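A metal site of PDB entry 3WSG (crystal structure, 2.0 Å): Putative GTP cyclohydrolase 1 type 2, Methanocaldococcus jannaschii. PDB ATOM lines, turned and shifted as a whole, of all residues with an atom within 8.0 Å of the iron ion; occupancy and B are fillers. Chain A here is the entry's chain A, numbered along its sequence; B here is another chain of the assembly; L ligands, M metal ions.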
ATOM      1  N   LEU A  52      10.811  22.505 -19.445  1.00  0.00           N
ATOM      2  CA  LEU A  52      11.380  22.165 -18.133  1.00  0.00           C
ATOM      3  C   LEU A  52      10.440  22.634 -17.016  1.00  0.00           C
ATOM      4  O   LEU A  52      10.052  21.847 -16.137  1.00  0.00           O
ATOM      5  CB  LEU A  52      12.750  22.801 -17.935  1.00  0.00           C
ATOM      6  CG  LEU A  52      13.518  22.356 -16.677  1.00  0.00           C
ATOM      7  CD1 LEU A  52      13.900  20.855 -16.804  1.00  0.00           C
ATOM      8  CD2 LEU A  52      14.743  23.193 -16.503  1.00  0.00           C
ATOM      9  N   ASP A  53      10.058  23.907 -17.095  1.00  0.00           N
ATOM     10  CA  ASP A  53       9.270  24.591 -16.050  1.00  0.00           C
ATOM     11  C   ASP A  53       7.891  25.035 -16.556  1.00  0.00           C
ATOM     12  O   ASP A  53       7.776  25.567 -17.676  1.00  0.00           O
ATOM     13  CB  ASP A  53       9.983  25.859 -15.554  1.00  0.00           C
ATOM     14  CG  ASP A  53      11.381  25.603 -15.069  1.00  0.00           C
ATOM     15  OD1 ASP A  53      11.549  24.772 -14.155  1.00  0.00           O
ATOM     16  OD2 ASP A  53      12.320  26.256 -15.587  1.00  0.00           O
ATOM     17  N   HIS A  73       8.671  18.978 -16.859  1.00  0.00           N
ATOM     18  CA  HIS A  73       9.416  18.139 -15.912  1.00  0.00           C
ATOM     19  C   HIS A  73       9.044  18.514 -14.468  1.00  0.00           C
ATOM     20  O   HIS A  73       8.733  17.632 -13.651  1.00  0.00           O
ATOM     21  CB  HIS A  73      10.926  18.280 -16.150  1.00  0.00           C
ATOM     22  CG  HIS A  73      11.787  17.466 -15.225  1.00  0.00           C
ATOM     23  ND1 HIS A  73      11.559  16.124 -14.963  1.00  0.00           N
ATOM     24  CD2 HIS A  73      12.908  17.789 -14.537  1.00  0.00           C
ATOM     25  CE1 HIS A  73      12.494  15.665 -14.150  1.00  0.00           C
ATOM     26  NE2 HIS A  73      13.323  16.658 -13.870  1.00  0.00           N
ATOM     27  N   HIS A  74       9.055  19.813 -14.143  1.00  0.00           N
ATOM     28  CA  HIS A  74       8.716  20.257 -12.772  1.00  0.00           C
ATOM     29  C   HIS A  74       7.214  20.439 -12.617  1.00  0.00           C
ATOM     30  O   HIS A  74       6.576  20.996 -13.494  1.00  0.00           O
ATOM     31  CB  HIS A  74       9.398  21.576 -12.427  1.00  0.00           C
ATOM     32  CG  HIS A  74      10.875  21.499 -12.527  1.00  0.00           C
ATOM     33  ND1 HIS A  74      11.615  22.416 -13.253  1.00  0.00           N
ATOM     34  CD2 HIS A  74      11.758  20.584 -12.069  1.00  0.00           C
ATOM     35  CE1 HIS A  74      12.892  22.090 -13.194  1.00  0.00           C
ATOM     36  NE2 HIS A  74      13.004  20.975 -12.502  1.00  0.00           N
ATOM     37  N   PRO A  75       6.657  19.990 -11.480  1.00  0.00           N
ATOM     38  CA  PRO A  75       5.230  20.171 -11.199  1.00  0.00           C
ATOM     39  C   PRO A  75       4.882  21.659 -11.082  1.00  0.00           C
ATOM     40  O   PRO A  75       5.752  22.471 -10.778  1.00  0.00           O
ATOM     41  CB  PRO A  75       5.023  19.449  -9.839  1.00  0.00           C
ATOM     42  CG  PRO A  75       6.181  18.476  -9.746  1.00  0.00           C
ATOM     43  CD  PRO A  75       7.345  19.167 -10.459  1.00  0.00           C
ATOM     44  N   HIS A 106       8.218  14.037 -13.148  1.00  0.00           N
ATOM     45  CA  HIS A 106       9.321  14.682 -12.472  1.00  0.00           C
ATOM     46  C   HIS A 106      10.348  13.598 -12.086  1.00  0.00           C
ATOM     47  O   HIS A 106      11.099  13.123 -12.942  1.00  0.00           O
ATOM     48  CB  HIS A 106       8.790  15.478 -11.256  1.00  0.00           C
ATOM     49  CG  HIS A 106       9.834  16.309 -10.572  1.00  0.00           C
ATOM     50  ND1 HIS A 106       9.780  16.598  -9.216  1.00  0.00           N
ATOM     51  CD2 HIS A 106      10.949  16.920 -11.041  1.00  0.00           C
ATOM     52  CE1 HIS A 106      10.832  17.334  -8.889  1.00  0.00           C
ATOM     53  NE2 HIS A 106      11.551  17.542  -9.982  1.00  0.00           N
ATOM     54  N   ASP A 110      13.385  11.327 -13.980  1.00  0.00           N
ATOM     55  CA  ASP A 110      14.773  11.306 -13.533  1.00  0.00           C
ATOM     56  C   ASP A 110      15.305   9.869 -13.411  1.00  0.00           C
ATOM     57  O   ASP A 110      16.464   9.600 -13.719  1.00  0.00           O
ATOM     58  CB  ASP A 110      14.928  11.976 -12.161  1.00  0.00           C
ATOM     59  CG  ASP A 110      14.765  13.502 -12.202  1.00  0.00           C
ATOM     60  OD1 ASP A 110      15.303  14.180 -13.091  1.00  0.00           O
ATOM     61  OD2 ASP A 110      14.072  14.026 -11.290  1.00  0.00           O
ATOM     62  N   LEU A 116      16.439  11.003 -17.297  1.00  0.00           N
ATOM     63  CA  LEU A 116      17.372  12.124 -17.330  1.00  0.00           C
ATOM     64  C   LEU A 116      18.754  11.759 -16.753  1.00  0.00           C
ATOM     65  O   LEU A 116      19.776  12.228 -17.250  1.00  0.00           O
ATOM     66  CB  LEU A 116      16.817  13.326 -16.546  1.00  0.00           C
ATOM     67  CG  LEU A 116      15.412  13.815 -16.936  1.00  0.00           C
ATOM     68  CD1 LEU A 116      15.138  15.147 -16.193  1.00  0.00           C
ATOM     69  CD2 LEU A 116      15.290  13.990 -18.447  1.00  0.00           C
ATOM     70  N   LEU A 179      23.849  13.760 -11.133  1.00  0.00           N
ATOM     71  CA  LEU A 179      22.467  13.912 -10.722  1.00  0.00           C
ATOM     72  C   LEU A 179      21.877  15.097 -11.488  1.00  0.00           C
ATOM     73  O   LEU A 179      22.331  16.220 -11.336  1.00  0.00           O
ATOM     74  CB  LEU A 179      22.399  14.122  -9.193  1.00  0.00           C
ATOM     75  CG  LEU A 179      21.069  14.172  -8.437  1.00  0.00           C
ATOM     76  CD1 LEU A 179      20.242  15.415  -8.776  1.00  0.00           C
ATOM     77  CD2 LEU A 179      20.283  12.953  -8.790  1.00  0.00           C
ATOM     78  N   SER A 180      20.852  14.816 -12.294  1.00  0.00           N
ATOM     79  CA  SER A 180      20.250  15.864 -13.126  1.00  0.00           C
ATOM     80  C   SER A 180      19.353  16.739 -12.272  1.00  0.00           C
ATOM     81  O   SER A 180      18.421  16.261 -11.626  1.00  0.00           O
ATOM     82  CB  SER A 180      19.427  15.256 -14.256  1.00  0.00           C
ATOM     83  OG  SER A 180      18.557  14.277 -13.730  1.00  0.00           O
ATOM     84  N   GLY A 181      19.641  18.019 -12.326  1.00  0.00           N
ATOM     85  CA  GLY A 181      18.856  19.000 -11.579  1.00  0.00           C
ATOM     86  C   GLY A 181      19.598  19.507 -10.344  1.00  0.00           C
ATOM     87  O   GLY A 181      20.775  19.832 -10.395  1.00  0.00           O
ATOM     88  N   TYR A 182      18.886  19.623  -9.234  1.00  0.00           N
ATOM     89  CA  TYR A 182      19.474  20.145  -8.000  1.00  0.00           C
ATOM     90  C   TYR A 182      19.974  19.001  -7.154  1.00  0.00           C
ATOM     91  O   TYR A 182      19.216  18.347  -6.433  1.00  0.00           O
ATOM     92  CB  TYR A 182      18.452  20.982  -7.221  1.00  0.00           C
ATOM     93  CG  TYR A 182      18.874  21.316  -5.806  1.00  0.00           C
ATOM     94  CD1 TYR A 182      20.131  21.853  -5.541  1.00  0.00           C
ATOM     95  CD2 TYR A 182      18.019  21.081  -4.741  1.00  0.00           C
ATOM     96  CE1 TYR A 182      20.530  22.149  -4.249  1.00  0.00           C
ATOM     97  CE2 TYR A 182      18.396  21.382  -3.440  1.00  0.00           C
ATOM     98  CZ  TYR A 182      19.657  21.918  -3.197  1.00  0.00           C
ATOM     99  OH  TYR A 182      20.036  22.214  -1.908  1.00  0.00           O
ATOM    100  N   GLY A 183      21.267  18.723  -7.227  1.00  0.00           N
ATOM    101  CA  GLY A 183      21.802  17.626  -6.453  1.00  0.00           C
ATOM    102  C   GLY A 183      22.838  18.069  -5.436  1.00  0.00           C
ATOM    103  O   GLY A 183      23.453  17.237  -4.791  1.00  0.00           O
ATOM    104  N   ASP A 203      22.959  23.775  -9.283  1.00  0.00           N
ATOM    105  CA  ASP A 203      22.491  24.652  -8.185  1.00  0.00           C
ATOM    106  C   ASP A 203      23.444  24.672  -6.955  1.00  0.00           C
ATOM    107  O   ASP A 203      23.021  24.455  -5.807  1.00  0.00           O
ATOM    108  CB  ASP A 203      21.057  24.266  -7.743  1.00  0.00           C
ATOM    109  CG  ASP A 203      19.944  25.022  -8.533  1.00  0.00           C
ATOM    110  OD1 ASP A 203      20.212  26.052  -9.223  1.00  0.00           O
ATOM    111  OD2 ASP A 203      18.768  24.597  -8.427  1.00  0.00           O
ATOM    112  N   HIS A 224      21.388  23.596 -12.907  1.00  0.00           N
ATOM    113  CA  HIS A 224      20.154  22.875 -12.771  1.00  0.00           C
ATOM    114  C   HIS A 224      19.471  22.721 -14.144  1.00  0.00           C
ATOM    115  O   HIS A 224      19.071  21.629 -14.551  1.00  0.00           O
ATOM    116  CB  HIS A 224      19.265  23.630 -11.791  1.00  0.00           C
ATOM    117  CG  HIS A 224      18.011  22.913 -11.421  1.00  0.00           C
ATOM    118  ND1 HIS A 224      17.422  23.051 -10.175  1.00  0.00           N
ATOM    119  CD2 HIS A 224      17.234  22.038 -12.105  1.00  0.00           C
ATOM    120  CE1 HIS A 224      16.330  22.307 -10.122  1.00  0.00           C
ATOM    121  NE2 HIS A 224      16.209  21.678 -11.278  1.00  0.00           N
ATOM    122  N   TYR A 225      19.351  23.830 -14.851  1.00  0.00           N
ATOM    123  CA  TYR A 225      18.690  23.836 -16.157  1.00  0.00           C
ATOM    124  C   TYR A 225      19.364  22.887 -17.158  1.00  0.00           C
ATOM    125  O   TYR A 225      18.712  21.989 -17.704  1.00  0.00           O
ATOM    126  CB  TYR A 225      18.649  25.258 -16.704  1.00  0.00           C
ATOM    127  CG  TYR A 225      18.152  25.428 -18.136  1.00  0.00           C
ATOM    128  CD1 TYR A 225      19.023  25.335 -19.226  1.00  0.00           C
ATOM    129  CD2 TYR A 225      16.803  25.750 -18.379  1.00  0.00           C
ATOM    130  CE1 TYR A 225      18.561  25.520 -20.532  1.00  0.00           C
ATOM    131  CE2 TYR A 225      16.327  25.926 -19.669  1.00  0.00           C
ATOM    132  CZ  TYR A 225      17.215  25.816 -20.742  1.00  0.00           C
ATOM    133  OH  TYR A 225      16.742  25.990 -21.999  1.00  0.00           O
ATOM    134  N   THR A 227      21.661  20.476 -16.866  1.00  0.00           N
ATOM    135  CA  THR A 227      21.824  19.051 -16.554  1.00  0.00           C
ATOM    136  C   THR A 227      20.498  18.289 -16.701  1.00  0.00           C
ATOM    137  O   THR A 227      20.509  17.061 -16.855  1.00  0.00           O
ATOM    138  CB  THR A 227      22.375  18.815 -15.131  1.00  0.00           C
ATOM    139  OG1 THR A 227      21.523  19.423 -14.156  1.00  0.00           O
ATOM    140  CG2 THR A 227      23.803  19.390 -15.004  1.00  0.00           C
ATOM    141  N   GLU A 228      19.376  19.007 -16.681  1.00  0.00           N
ATOM    142  CA  GLU A 228      18.077  18.366 -16.970  1.00  0.00           C
ATOM    143  C   GLU A 228      17.676  18.460 -18.451  1.00  0.00           C
ATOM    144  O   GLU A 228      17.098  17.532 -19.008  1.00  0.00           O
ATOM    145  CB  GLU A 228      16.982  18.981 -16.107  1.00  0.00           C
ATOM    146  CG  GLU A 228      17.040  18.470 -14.675  1.00  0.00           C
ATOM    147  CD  GLU A 228      16.056  19.155 -13.814  1.00  0.00           C
ATOM    148  OE1 GLU A 228      15.555  20.261 -14.173  1.00  0.00           O
ATOM    149  OE2 GLU A 228      15.813  18.576 -12.741  1.00  0.00           O
ATOM    150  N   HIS B 206      18.028  27.852  -9.518  1.00  0.00           N
ATOM    151  CA  HIS B 206      17.137  27.855 -10.658  1.00  0.00           C
ATOM    152  C   HIS B 206      15.673  28.242 -10.333  1.00  0.00           C
ATOM    153  O   HIS B 206      15.127  29.147 -10.974  1.00  0.00           O
ATOM    154  CB  HIS B 206      17.131  26.479 -11.331  1.00  0.00           C
ATOM    155  CG  HIS B 206      16.234  26.408 -12.529  1.00  0.00           C
ATOM    156  ND1 HIS B 206      16.492  27.095 -13.694  1.00  0.00           N
ATOM    157  CD2 HIS B 206      15.057  25.773 -12.722  1.00  0.00           C
ATOM    158  CE1 HIS B 206      15.530  26.861 -14.565  1.00  0.00           C
ATOM    159  NE2 HIS B 206      14.646  26.050 -13.998  1.00  0.00           N
ATOM    160  N   HIS B 207      15.046  27.570  -9.358  1.00  0.00           N
ATOM    161  CA  HIS B 207      13.621  27.826  -9.098  1.00  0.00           C
ATOM    162  C   HIS B 207      13.402  29.272  -8.672  1.00  0.00           C
ATOM    163  O   HIS B 207      12.398  29.869  -9.043  1.00  0.00           O
ATOM    164  CB  HIS B 207      13.026  26.881  -8.042  1.00  0.00           C
ATOM    165  CG  HIS B 207      12.931  25.445  -8.481  1.00  0.00           C
ATOM    166  ND1 HIS B 207      12.405  25.064  -9.693  1.00  0.00           N
ATOM    167  CD2 HIS B 207      13.260  24.293  -7.841  1.00  0.00           C
ATOM    168  CE1 HIS B 207      12.418  23.749  -9.797  1.00  0.00           C
ATOM    169  NE2 HIS B 207      12.940  23.257  -8.677  1.00  0.00           N
HETATM  170  C1  LIG L   1      15.827  16.090  -8.851  1.00  0.00           C
HETATM  171  O1  LIG L   1      15.615  14.869  -8.686  1.00  0.00           O
HETATM  172  O2  LIG L   1      16.046  16.493 -10.032  1.00  0.00           O
HETATM  173  C2  LIG L   1      15.844  17.023  -7.641  1.00  0.00           C
HETATM  174  C3  LIG L   1      14.909  18.230  -7.705  1.00  0.00           C
HETATM  175  O3  LIG L   1      13.564  17.853  -7.532  1.00  0.00           O
HETATM  176  C4  LIG L   1      15.295  19.199  -6.595  1.00  0.00           C
HETATM  177  C5  LIG L   1      14.472  20.472  -6.527  1.00  0.00           C
HETATM  178  O4  LIG L   1      13.991  21.009  -7.561  1.00  0.00           O
HETATM  179  O5  LIG L   1      14.264  21.030  -5.402  1.00  0.00           O
HETATM  180  C6  LIG L   1      15.058  18.870  -9.069  1.00  0.00           C
HETATM  181  O6  LIG L   1      16.197  19.186  -9.513  1.00  0.00           O
HETATM  182  O7  LIG L   1      14.025  19.059  -9.771  1.00  0.00           O
HETATM  183 FE    FE M   1      14.763  20.075 -11.549  1.00  0.00          FE
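Of the 20 residues printed, 3 come within 4 Å of the iron ion.
ND1 of His 74 lies within hydrogen-bond range of OD1 of Asp 53 (2.5 Å).
The backbone carbonyl oxygen (O) of His 224 sits at hydrogen-bond distance from the side-chain hydroxyl (OG1) of Thr 227, at 3.3 Å.
A ring nitrogen (ND1) of His 224 sits at hydrogen-bond distance from the side-chain carboxylate (OD2) of Asp 203 (2.7 Å).
The side-chain carboxylate (OE2) of Glu 228 lies close to a ring nitrogen (NE2) of His 73 (3.3 Å).
N of His 74 sits at hydrogen-bond distance from O of Leu 52 (3.0 Å).
The iron ion is bound by NE2 of His 224 (2.2 Å), O7 of the ligand (2.2 Å), OE2 of Glu 228 (2.2 Å) and NE2 of His 74 (2.2 Å).
The iron ion has four donor atoms within binding distance.
Slightly farther from the iron ion lies an oxygen (O6) of the ligand (2.6 Å).
Slightly farther from the iron ion lies the side-chain carboxylate (OE1) of Glu 228 (2.7 Å).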
